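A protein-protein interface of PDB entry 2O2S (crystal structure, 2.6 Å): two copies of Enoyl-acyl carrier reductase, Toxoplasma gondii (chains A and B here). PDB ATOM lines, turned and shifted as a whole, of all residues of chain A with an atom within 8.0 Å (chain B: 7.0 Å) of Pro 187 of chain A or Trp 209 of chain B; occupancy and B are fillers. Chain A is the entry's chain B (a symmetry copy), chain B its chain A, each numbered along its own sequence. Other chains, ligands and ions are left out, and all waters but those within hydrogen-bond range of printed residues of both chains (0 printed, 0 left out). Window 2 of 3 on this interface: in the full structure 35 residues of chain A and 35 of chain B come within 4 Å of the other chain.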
ATOM      1  N   VAL A 134      28.746 -10.841  39.635  1.00  0.00           N
ATOM      2  CA  VAL A 134      27.568 -10.393  38.861  1.00  0.00           C
ATOM      3  C   VAL A 134      27.850  -9.869  37.429  1.00  0.00           C
ATOM      4  O   VAL A 134      26.991 -10.003  36.535  1.00  0.00           O
ATOM      5  CB  VAL A 134      26.757  -9.327  39.626  1.00  0.00           C
ATOM      6  CG1 VAL A 134      27.609  -8.072  39.902  1.00  0.00           C
ATOM      7  CG2 VAL A 134      25.471  -8.973  38.872  1.00  0.00           C
ATOM      8  N   PRO A 137      29.236 -12.984  32.544  1.00  0.00           N
ATOM      9  CA  PRO A 137      28.182 -13.875  32.098  1.00  0.00           C
ATOM     10  C   PRO A 137      28.440 -15.309  32.582  1.00  0.00           C
ATOM     11  O   PRO A 137      29.549 -15.647  33.042  1.00  0.00           O
ATOM     12  CB  PRO A 137      28.257 -13.758  30.568  1.00  0.00           C
ATOM     13  CG  PRO A 137      29.664 -13.442  30.298  1.00  0.00           C
ATOM     14  CD  PRO A 137      30.103 -12.560  31.433  1.00  0.00           C
ATOM     15  N   LEU A 139      28.818 -18.188  31.315  1.00  0.00           N
ATOM     16  CA  LEU A 139      29.945 -18.942  30.747  1.00  0.00           C
ATOM     17  C   LEU A 139      31.291 -18.567  31.366  1.00  0.00           C
ATOM     18  O   LEU A 139      32.246 -19.275  31.169  1.00  0.00           O
ATOM     19  CB  LEU A 139      30.020 -18.755  29.231  1.00  0.00           C
ATOM     20  CG  LEU A 139      28.984 -19.550  28.457  1.00  0.00           C
ATOM     21  CD1 LEU A 139      28.882 -19.058  27.025  1.00  0.00           C
ATOM     22  CD2 LEU A 139      29.345 -21.013  28.525  1.00  0.00           C
ATOM     23  N   TYR A 179      14.154 -10.887  40.661  1.00  0.00           N
ATOM     24  CA  TYR A 179      14.183 -10.147  39.431  1.00  0.00           C
ATOM     25  C   TYR A 179      13.868 -11.073  38.252  1.00  0.00           C
ATOM     26  O   TYR A 179      14.147 -12.280  38.274  1.00  0.00           O
ATOM     27  CB  TYR A 179      15.549  -9.461  39.300  1.00  0.00           C
ATOM     28  CG  TYR A 179      15.682  -8.622  38.065  1.00  0.00           C
ATOM     29  CD1 TYR A 179      14.764  -7.612  37.794  1.00  0.00           C
ATOM     30  CD2 TYR A 179      16.721  -8.844  37.160  1.00  0.00           C
ATOM     31  CE1 TYR A 179      14.873  -6.850  36.664  1.00  0.00           C
ATOM     32  CE2 TYR A 179      16.840  -8.099  36.035  1.00  0.00           C
ATOM     33  CZ  TYR A 179      15.918  -7.095  35.784  1.00  0.00           C
ATOM     34  OH  TYR A 179      16.037  -6.342  34.635  1.00  0.00           O
ATOM     35  N   ALA A 181      15.175 -11.798  35.530  1.00  0.00           N
ATOM     36  CA  ALA A 181      16.254 -12.721  35.179  1.00  0.00           C
ATOM     37  C   ALA A 181      16.035 -14.188  35.639  1.00  0.00           C
ATOM     38  O   ALA A 181      16.445 -15.140  34.979  1.00  0.00           O
ATOM     39  CB  ALA A 181      17.569 -12.193  35.744  1.00  0.00           C
ATOM     40  N   ARG A 184      13.357 -15.283  32.876  1.00  0.00           N
ATOM     41  CA  ARG A 184      13.754 -15.028  31.503  1.00  0.00           C
ATOM     42  C   ARG A 184      15.097 -14.304  31.402  1.00  0.00           C
ATOM     43  O   ARG A 184      15.430 -13.486  32.260  1.00  0.00           O
ATOM     44  CB  ARG A 184      12.668 -14.221  30.823  1.00  0.00           C
ATOM     45  CG  ARG A 184      11.569 -15.046  30.160  1.00  0.00           C
ATOM     46  CD  ARG A 184      10.477 -14.125  29.567  1.00  0.00           C
ATOM     47  NE  ARG A 184       9.417 -13.940  30.550  1.00  0.00           N
ATOM     48  CZ  ARG A 184       8.638 -12.865  30.709  1.00  0.00           C
ATOM     49  NH1 ARG A 184       8.733 -11.781  29.945  1.00  0.00           N
ATOM     50  NH2 ARG A 184       7.723 -12.895  31.673  1.00  0.00           N
ATOM     51  N   VAL A 185      15.836 -14.603  30.324  1.00  0.00           N
ATOM     52  CA  VAL A 185      17.167 -14.079  30.126  1.00  0.00           C
ATOM     53  C   VAL A 185      17.201 -12.567  30.076  1.00  0.00           C
ATOM     54  O   VAL A 185      16.458 -11.934  29.324  1.00  0.00           O
ATOM     55  CB  VAL A 185      17.857 -14.621  28.881  1.00  0.00           C
ATOM     56  CG1 VAL A 185      19.349 -14.210  28.904  1.00  0.00           C
ATOM     57  CG2 VAL A 185      17.754 -16.167  28.827  1.00  0.00           C
ATOM     58  N   VAL A 186      18.051 -12.027  30.949  1.00  0.00           N
ATOM     59  CA  VAL A 186      18.429 -10.638  31.019  1.00  0.00           C
ATOM     60  C   VAL A 186      19.959 -10.516  30.919  1.00  0.00           C
ATOM     61  O   VAL A 186      20.694 -10.836  31.873  1.00  0.00           O
ATOM     62  CB  VAL A 186      17.965 -10.044  32.320  1.00  0.00           C
ATOM     63  CG1 VAL A 186      18.533  -8.649  32.509  1.00  0.00           C
ATOM     64  CG2 VAL A 186      16.445 -10.016  32.344  1.00  0.00           C
ATOM     65  N   PRO A 187      20.452 -10.076  29.740  1.00  0.00           N
ATOM     66  CA  PRO A 187      21.897  -9.832  29.580  1.00  0.00           C
ATOM     67  C   PRO A 187      22.381  -8.781  30.556  1.00  0.00           C
ATOM     68  O   PRO A 187      21.667  -7.770  30.832  1.00  0.00           O
ATOM     69  CB  PRO A 187      22.023  -9.342  28.149  1.00  0.00           C
ATOM     70  CG  PRO A 187      20.837  -9.941  27.453  1.00  0.00           C
ATOM     71  CD  PRO A 187      19.733  -9.844  28.478  1.00  0.00           C
ATOM     72  N   GLY A 188      23.555  -9.081  31.113  1.00  0.00           N
ATOM     73  CA  GLY A 188      24.226  -8.230  32.079  1.00  0.00           C
ATOM     74  C   GLY A 188      24.042  -8.644  33.522  1.00  0.00           C
ATOM     75  O   GLY A 188      24.856  -8.264  34.349  1.00  0.00           O
ATOM     76  N   TYR A 189      22.960  -9.383  33.822  1.00  0.00           N
ATOM     77  CA  TYR A 189      22.648  -9.841  35.182  1.00  0.00           C
ATOM     78  C   TYR A 189      23.328 -11.194  35.469  1.00  0.00           C
ATOM     79  O   TYR A 189      22.655 -12.200  35.630  1.00  0.00           O
ATOM     80  CB  TYR A 189      21.124  -9.975  35.360  1.00  0.00           C
ATOM     81  CG  TYR A 189      20.650 -10.141  36.794  1.00  0.00           C
ATOM     82  CD1 TYR A 189      20.611  -9.061  37.644  1.00  0.00           C
ATOM     83  CD2 TYR A 189      20.234 -11.383  37.293  1.00  0.00           C
ATOM     84  CE1 TYR A 189      20.197  -9.183  38.948  1.00  0.00           C
ATOM     85  CE2 TYR A 189      19.785 -11.527  38.614  1.00  0.00           C
ATOM     86  CZ  TYR A 189      19.771 -10.416  39.442  1.00  0.00           C
ATOM     87  OH  TYR A 189      19.333 -10.486  40.769  1.00  0.00           O
ATOM     88  N   GLY A 190      24.649 -11.212  35.551  1.00  0.00           N
ATOM     89  CA  GLY A 190      25.402 -12.468  35.531  1.00  0.00           C
ATOM     90  C   GLY A 190      25.771 -12.956  36.900  1.00  0.00           C
ATOM     91  O   GLY A 190      25.130 -12.610  37.882  1.00  0.00           O
ATOM     92  N   PHE A 243      24.824  -0.963  33.872  1.00  0.00           N
ATOM     93  CA  PHE A 243      23.709  -1.895  33.861  1.00  0.00           C
ATOM     94  C   PHE A 243      22.373  -1.299  34.247  1.00  0.00           C
ATOM     95  O   PHE A 243      21.408  -1.424  33.524  1.00  0.00           O
ATOM     96  CB  PHE A 243      23.990  -3.069  34.798  1.00  0.00           C
ATOM     97  CG  PHE A 243      22.947  -4.123  34.741  1.00  0.00           C
ATOM     98  CD1 PHE A 243      22.958  -5.070  33.719  1.00  0.00           C
ATOM     99  CD2 PHE A 243      21.925  -4.149  35.666  1.00  0.00           C
ATOM    100  CE1 PHE A 243      21.988  -6.033  33.632  1.00  0.00           C
ATOM    101  CE2 PHE A 243      20.945  -5.121  35.593  1.00  0.00           C
ATOM    102  CZ  PHE A 243      20.987  -6.070  34.566  1.00  0.00           C
ATOM    103  N   TYR A 246      20.798   1.575  32.009  1.00  0.00           N
ATOM    104  CA  TYR A 246      20.140   1.022  30.818  1.00  0.00           C
ATOM    105  C   TYR A 246      18.869   0.234  31.129  1.00  0.00           C
ATOM    106  O   TYR A 246      17.891   0.280  30.373  1.00  0.00           O
ATOM    107  CB  TYR A 246      21.110   0.146  30.013  1.00  0.00           C
ATOM    108  CG  TYR A 246      22.225   0.935  29.348  1.00  0.00           C
ATOM    109  CD1 TYR A 246      23.571   0.570  29.495  1.00  0.00           C
ATOM    110  CD2 TYR A 246      21.931   2.067  28.583  1.00  0.00           C
ATOM    111  CE1 TYR A 246      24.594   1.308  28.869  1.00  0.00           C
ATOM    112  CE2 TYR A 246      22.931   2.800  27.968  1.00  0.00           C
ATOM    113  CZ  TYR A 246      24.256   2.426  28.108  1.00  0.00           C
ATOM    114  OH  TYR A 246      25.214   3.205  27.475  1.00  0.00           O
ATOM    115  N   ALA A 247      18.887  -0.492  32.245  1.00  0.00           N
ATOM    116  CA  ALA A 247      17.700  -1.201  32.725  1.00  0.00           C
ATOM    117  C   ALA A 247      16.540  -0.248  32.903  1.00  0.00           C
ATOM    118  O   ALA A 247      15.429  -0.512  32.448  1.00  0.00           O
ATOM    119  CB  ALA A 247      17.999  -1.897  34.050  1.00  0.00           C
ATOM    120  N   ASP B 203      19.216 -21.686  34.234  1.00  0.00           N
ATOM    121  CA  ASP B 203      20.493 -21.626  33.526  1.00  0.00           C
ATOM    122  C   ASP B 203      20.377 -22.157  32.107  1.00  0.00           C
ATOM    123  O   ASP B 203      21.093 -21.737  31.190  1.00  0.00           O
ATOM    124  CB  ASP B 203      21.583 -22.380  34.285  1.00  0.00           C
ATOM    125  CG  ASP B 203      21.907 -21.734  35.612  1.00  0.00           C
ATOM    126  OD1 ASP B 203      21.458 -20.598  35.848  1.00  0.00           O
ATOM    127  OD2 ASP B 203      22.607 -22.355  36.426  1.00  0.00           O
ATOM    128  N   THR B 204      19.478 -23.092  31.925  1.00  0.00           N
ATOM    129  CA  THR B 204      19.203 -23.641  30.604  1.00  0.00           C
ATOM    130  C   THR B 204      18.786 -22.482  29.676  1.00  0.00           C
ATOM    131  O   THR B 204      19.292 -22.330  28.587  1.00  0.00           O
ATOM    132  CB  THR B 204      18.151 -24.793  30.760  1.00  0.00           C
ATOM    133  OG1 THR B 204      18.758 -25.856  31.501  1.00  0.00           O
ATOM    134  CG2 THR B 204      17.647 -25.331  29.430  1.00  0.00           C
ATOM    135  N   ARG B 205      17.933 -21.604  30.166  1.00  0.00           N
ATOM    136  CA  ARG B 205      17.488 -20.456  29.388  1.00  0.00           C
ATOM    137  C   ARG B 205      18.618 -19.495  29.136  1.00  0.00           C
ATOM    138  O   ARG B 205      18.833 -19.048  28.017  1.00  0.00           O
ATOM    139  CB  ARG B 205      16.363 -19.771  30.130  1.00  0.00           C
ATOM    140  CG  ARG B 205      15.140 -20.634  30.163  1.00  0.00           C
ATOM    141  CD  ARG B 205      13.898 -19.881  30.641  1.00  0.00           C
ATOM    142  NE  ARG B 205      13.963 -19.573  32.074  1.00  0.00           N
ATOM    143  CZ  ARG B 205      13.626 -20.421  33.048  1.00  0.00           C
ATOM    144  NH1 ARG B 205      13.207 -21.631  32.781  1.00  0.00           N
ATOM    145  NH2 ARG B 205      13.717 -20.039  34.307  1.00  0.00           N
ATOM    146  N   THR B 206      19.353 -19.181  30.193  1.00  0.00           N
ATOM    147  CA  THR B 206      20.387 -18.167  30.128  1.00  0.00           C
ATOM    148  C   THR B 206      21.539 -18.623  29.233  1.00  0.00           C
ATOM    149  O   THR B 206      21.946 -17.889  28.344  1.00  0.00           O
ATOM    150  CB  THR B 206      20.827 -17.795  31.550  1.00  0.00           C
ATOM    151  OG1 THR B 206      19.676 -17.314  32.269  1.00  0.00           O
ATOM    152  CG2 THR B 206      21.905 -16.709  31.538  1.00  0.00           C
ATOM    153  N   LEU B 207      22.026 -19.848  29.473  1.00  0.00           N
ATOM    154  CA  LEU B 207      22.998 -20.534  28.615  1.00  0.00           C
ATOM    155  C   LEU B 207      22.490 -20.761  27.187  1.00  0.00           C
ATOM    156  O   LEU B 207      23.270 -20.698  26.239  1.00  0.00           O
ATOM    157  CB  LEU B 207      23.382 -21.921  29.202  1.00  0.00           C
ATOM    158  CG  LEU B 207      24.263 -22.056  30.457  1.00  0.00           C
ATOM    159  CD1 LEU B 207      24.143 -23.463  31.050  1.00  0.00           C
ATOM    160  CD2 LEU B 207      25.750 -21.722  30.178  1.00  0.00           C
ATOM    161  N   ALA B 208      21.211 -21.081  27.012  1.00  0.00           N
ATOM    162  CA  ALA B 208      20.704 -21.206  25.633  1.00  0.00           C
ATOM    163  C   ALA B 208      20.973 -19.916  24.852  1.00  0.00           C
ATOM    164  O   ALA B 208      21.319 -19.986  23.656  1.00  0.00           O
ATOM    165  CB  ALA B 208      19.192 -21.570  25.587  1.00  0.00           C
ATOM    166  N   TRP B 209      20.801 -18.767  25.527  1.00  0.00           N
ATOM    167  CA  TRP B 209      21.193 -17.470  25.001  1.00  0.00           C
ATOM    168  C   TRP B 209      22.689 -17.407  24.823  1.00  0.00           C
ATOM    169  O   TRP B 209      23.183 -17.219  23.717  1.00  0.00           O
ATOM    170  CB  TRP B 209      20.759 -16.354  25.940  1.00  0.00           C
ATOM    171  CG  TRP B 209      21.392 -15.011  25.725  1.00  0.00           C
ATOM    172  CD1 TRP B 209      22.194 -14.327  26.605  1.00  0.00           C
ATOM    173  CD2 TRP B 209      21.244 -14.158  24.577  1.00  0.00           C
ATOM    174  NE1 TRP B 209      22.558 -13.101  26.070  1.00  0.00           N
ATOM    175  CE2 TRP B 209      21.991 -12.976  24.829  1.00  0.00           C
ATOM    176  CE3 TRP B 209      20.559 -14.280  23.364  1.00  0.00           C
ATOM    177  CZ2 TRP B 209      22.080 -11.931  23.899  1.00  0.00           C
ATOM    178  CZ3 TRP B 209      20.639 -13.231  22.438  1.00  0.00           C
ATOM    179  CH2 TRP B 209      21.401 -12.074  22.711  1.00  0.00           C
ATOM    180  N   GLU B 210      23.420 -17.563  25.912  1.00  0.00           N
ATOM    181  CA  GLU B 210      24.862 -17.365  25.860  1.00  0.00           C
ATOM    182  C   GLU B 210      25.502 -18.313  24.851  1.00  0.00           C
ATOM    183  O   GLU B 210      26.059 -17.852  23.857  1.00  0.00           O
ATOM    184  CB  GLU B 210      25.509 -17.514  27.246  1.00  0.00           C
ATOM    185  CG  GLU B 210      25.160 -16.398  28.204  1.00  0.00           C
ATOM    186  CD  GLU B 210      26.047 -16.383  29.420  1.00  0.00           C
ATOM    187  OE1 GLU B 210      27.114 -17.058  29.426  1.00  0.00           O
ATOM    188  OE2 GLU B 210      25.663 -15.697  30.384  1.00  0.00           O
ATOM    189  N   ALA B 211      25.386 -19.615  25.075  1.00  0.00           N
ATOM    190  CA  ALA B 211      25.921 -20.602  24.130  1.00  0.00           C
ATOM    191  C   ALA B 211      25.317 -20.543  22.722  1.00  0.00           C
ATOM    192  O   ALA B 211      26.008 -20.802  21.734  1.00  0.00           O
ATOM    193  CB  ALA B 211      25.781 -22.012  24.691  1.00  0.00           C
ATOM    194  N   GLY B 212      24.037 -20.234  22.618  1.00  0.00           N
ATOM    195  CA  GLY B 212      23.428 -19.996  21.300  1.00  0.00           C
ATOM    196  C   GLY B 212      24.041 -18.839  20.507  1.00  0.00           C
ATOM    197  O   GLY B 212      24.270 -18.976  19.323  1.00  0.00           O
ATOM    198  N   GLN B 213      24.312 -17.711  21.165  1.00  0.00           N
ATOM    199  CA  GLN B 213      24.979 -16.555  20.528  1.00  0.00           C
ATOM    200  C   GLN B 213      26.479 -16.804  20.226  1.00  0.00           C
ATOM    201  O   GLN B 213      26.944 -16.564  19.131  1.00  0.00           O
ATOM    202  CB  GLN B 213      24.813 -15.302  21.384  1.00  0.00           C
ATOM    203  CG  GLN B 213      23.392 -14.730  21.403  1.00  0.00           C
ATOM    204  CD  GLN B 213      23.068 -13.986  20.132  1.00  0.00           C
ATOM    205  OE1 GLN B 213      23.683 -12.967  19.833  1.00  0.00           O
ATOM    206  NE2 GLN B 213      22.110 -14.488  19.371  1.00  0.00           N
ATOM    207  N   LYS B 214      27.222 -17.313  21.184  1.00  0.00           N
ATOM    208  CA  LYS B 214      28.640 -17.545  20.990  1.00  0.00           C
ATOM    209  C   LYS B 214      28.929 -18.748  20.100  1.00  0.00           C
ATOM    210  O   LYS B 214      29.625 -18.603  19.110  1.00  0.00           O
ATOM    211  CB  LYS B 214      29.324 -17.736  22.333  1.00  0.00           C
ATOM    212  CG  LYS B 214      30.823 -17.651  22.266  1.00  0.00           C
ATOM    213  CD  LYS B 214      31.430 -17.757  23.644  1.00  0.00           C
ATOM    214  CE  LYS B 214      32.912 -17.439  23.612  1.00  0.00           C
ATOM    215  NZ  LYS B 214      33.587 -18.053  24.780  1.00  0.00           N
ATOM    216  N   TYR B 215      28.407 -19.922  20.451  1.00  0.00           N
ATOM    217  CA  TYR B 215      28.699 -21.177  19.719  1.00  0.00           C
ATOM    218  C   TYR B 215      27.626 -21.649  18.719  1.00  0.00           C
ATOM    219  O   TYR B 215      27.872 -22.556  17.955  1.00  0.00           O
ATOM    220  CB  TYR B 215      28.941 -22.317  20.711  1.00  0.00           C
ATOM    221  CG  TYR B 215      30.035 -22.041  21.736  1.00  0.00           C
ATOM    222  CD1 TYR B 215      29.756 -22.043  23.100  1.00  0.00           C
ATOM    223  CD2 TYR B 215      31.347 -21.768  21.335  1.00  0.00           C
ATOM    224  CE1 TYR B 215      30.738 -21.775  24.020  1.00  0.00           C
ATOM    225  CE2 TYR B 215      32.332 -21.517  22.256  1.00  0.00           C
ATOM    226  CZ  TYR B 215      32.017 -21.521  23.590  1.00  0.00           C
ATOM    227  OH  TYR B 215      32.996 -21.281  24.504  1.00  0.00           O
ATOM    228  N   VAL B 217      25.115 -23.165  19.716  1.00  0.00           N
ATOM    229  CA  VAL B 217      24.750 -24.387  20.393  1.00  0.00           C
ATOM    230  C   VAL B 217      23.361 -24.179  21.031  1.00  0.00           C
ATOM    231  O   VAL B 217      22.995 -23.052  21.480  1.00  0.00           O
ATOM    232  CB  VAL B 217      25.807 -24.748  21.481  1.00  0.00           C
ATOM    233  CG1 VAL B 217      25.297 -25.835  22.397  1.00  0.00           C
ATOM    234  CG2 VAL B 217      27.151 -25.176  20.837  1.00  0.00           C
ATOM    235  N   VAL B 219      20.562 -25.543  23.875  1.00  0.00           N
ATOM    236  CA  VAL B 219      20.594 -25.929  25.247  1.00  0.00           C
ATOM    237  C   VAL B 219      19.151 -26.112  25.707  1.00  0.00           C
ATOM    238  O   VAL B 219      18.365 -25.164  25.692  1.00  0.00           O
ATOM    239  CB  VAL B 219      21.276 -24.820  26.120  1.00  0.00           C
ATOM    240  CG1 VAL B 219      21.647 -25.360  27.503  1.00  0.00           C
ATOM    241  CG2 VAL B 219      22.537 -24.283  25.436  1.00  0.00           C
ATOM    242  N   SER B 282      15.376 -24.332  21.514  1.00  0.00           N
ATOM    243  CA  SER B 282      16.391 -24.072  22.515  1.00  0.00           C
ATOM    244  C   SER B 282      15.793 -23.317  23.704  1.00  0.00           C
ATOM    245  O   SER B 282      14.840 -22.543  23.563  1.00  0.00           O
ATOM    246  CB  SER B 282      17.569 -23.311  21.906  1.00  0.00           C
ATOM    247  OG  SER B 282      18.651 -23.275  22.799  1.00  0.00           O
ATOM    248  N   GLY B 283      16.381 -23.565  24.878  1.00  0.00           N
ATOM    249  CA  GLY B 283      15.976 -22.908  26.129  1.00  0.00           C
ATOM    250  C   GLY B 283      14.687 -23.420  26.775  1.00  0.00           C
ATOM    251  O   GLY B 283      14.160 -22.768  27.656  1.00  0.00           O
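The side-chain carboxylate (OE1) of Glu 210 of chain B sits at hydrogen-bond distance from the backbone NH (N) of Leu 139 of chain A, 2.8 Å away.
Among the printed residues, pairs that only touch across the chains: Val 185 of chain A with Arg 205 of chain B (3.2 Å), Pro 137 of chain A with Glu 210 of chain B (3.2 Å), Val 185 of chain A with Thr 206 of chain B (3.6 Å), Val 185 of chain A with Trp 209 of chain B (3.7 Å) and Pro 187 of chain A with Trp 209 of chain B (3.9 Å).
Printed residues of chain B within 4 Å of Leu 139 of chain A: Glu 210.
Of the printed residues of chain A, Thr 206 of chain B touches Val 185.
Ala 208 of chain B touches none of the printed residues of chain A.
Of chain A, only Val 185 (3.7 Å) and Pro 187 (3.9 Å) come within 4 Å of Trp 209 of chain B.
Of the printed residues of chain A, Glu 210 of chain B touches Pro 137 and Leu 139.
The nearest printed residue of chain B that does not touch Pro 187 of chain A is Glu 210 of chain B (7.0 Å).
Of the 15 printed residues of chain A, 4 touch a printed residue of chain B.
Printed residues of chain A that touch a printed residue of chain B: Pro 137, Leu 139, Val 185 and Pro 187.
Hydrophobic or aromatic side chains of chain A that line the printed part of chain B: Pro 137, Leu 139, Val 185 and Pro 187.
Hydrophobic or aromatic side chains of chain B within 4 Å of the printed part of chain A: Trp 209.
Along chain B the printed residues that touch a printed residue of chain A span positions 205 to 210.
Among the printed residues, 6 pairs touch across the chains.
No position is printed for both chains.
Of the 6 pairs that touch across the chains among the printed residues, none has its exchanged pair printed and touching as well.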
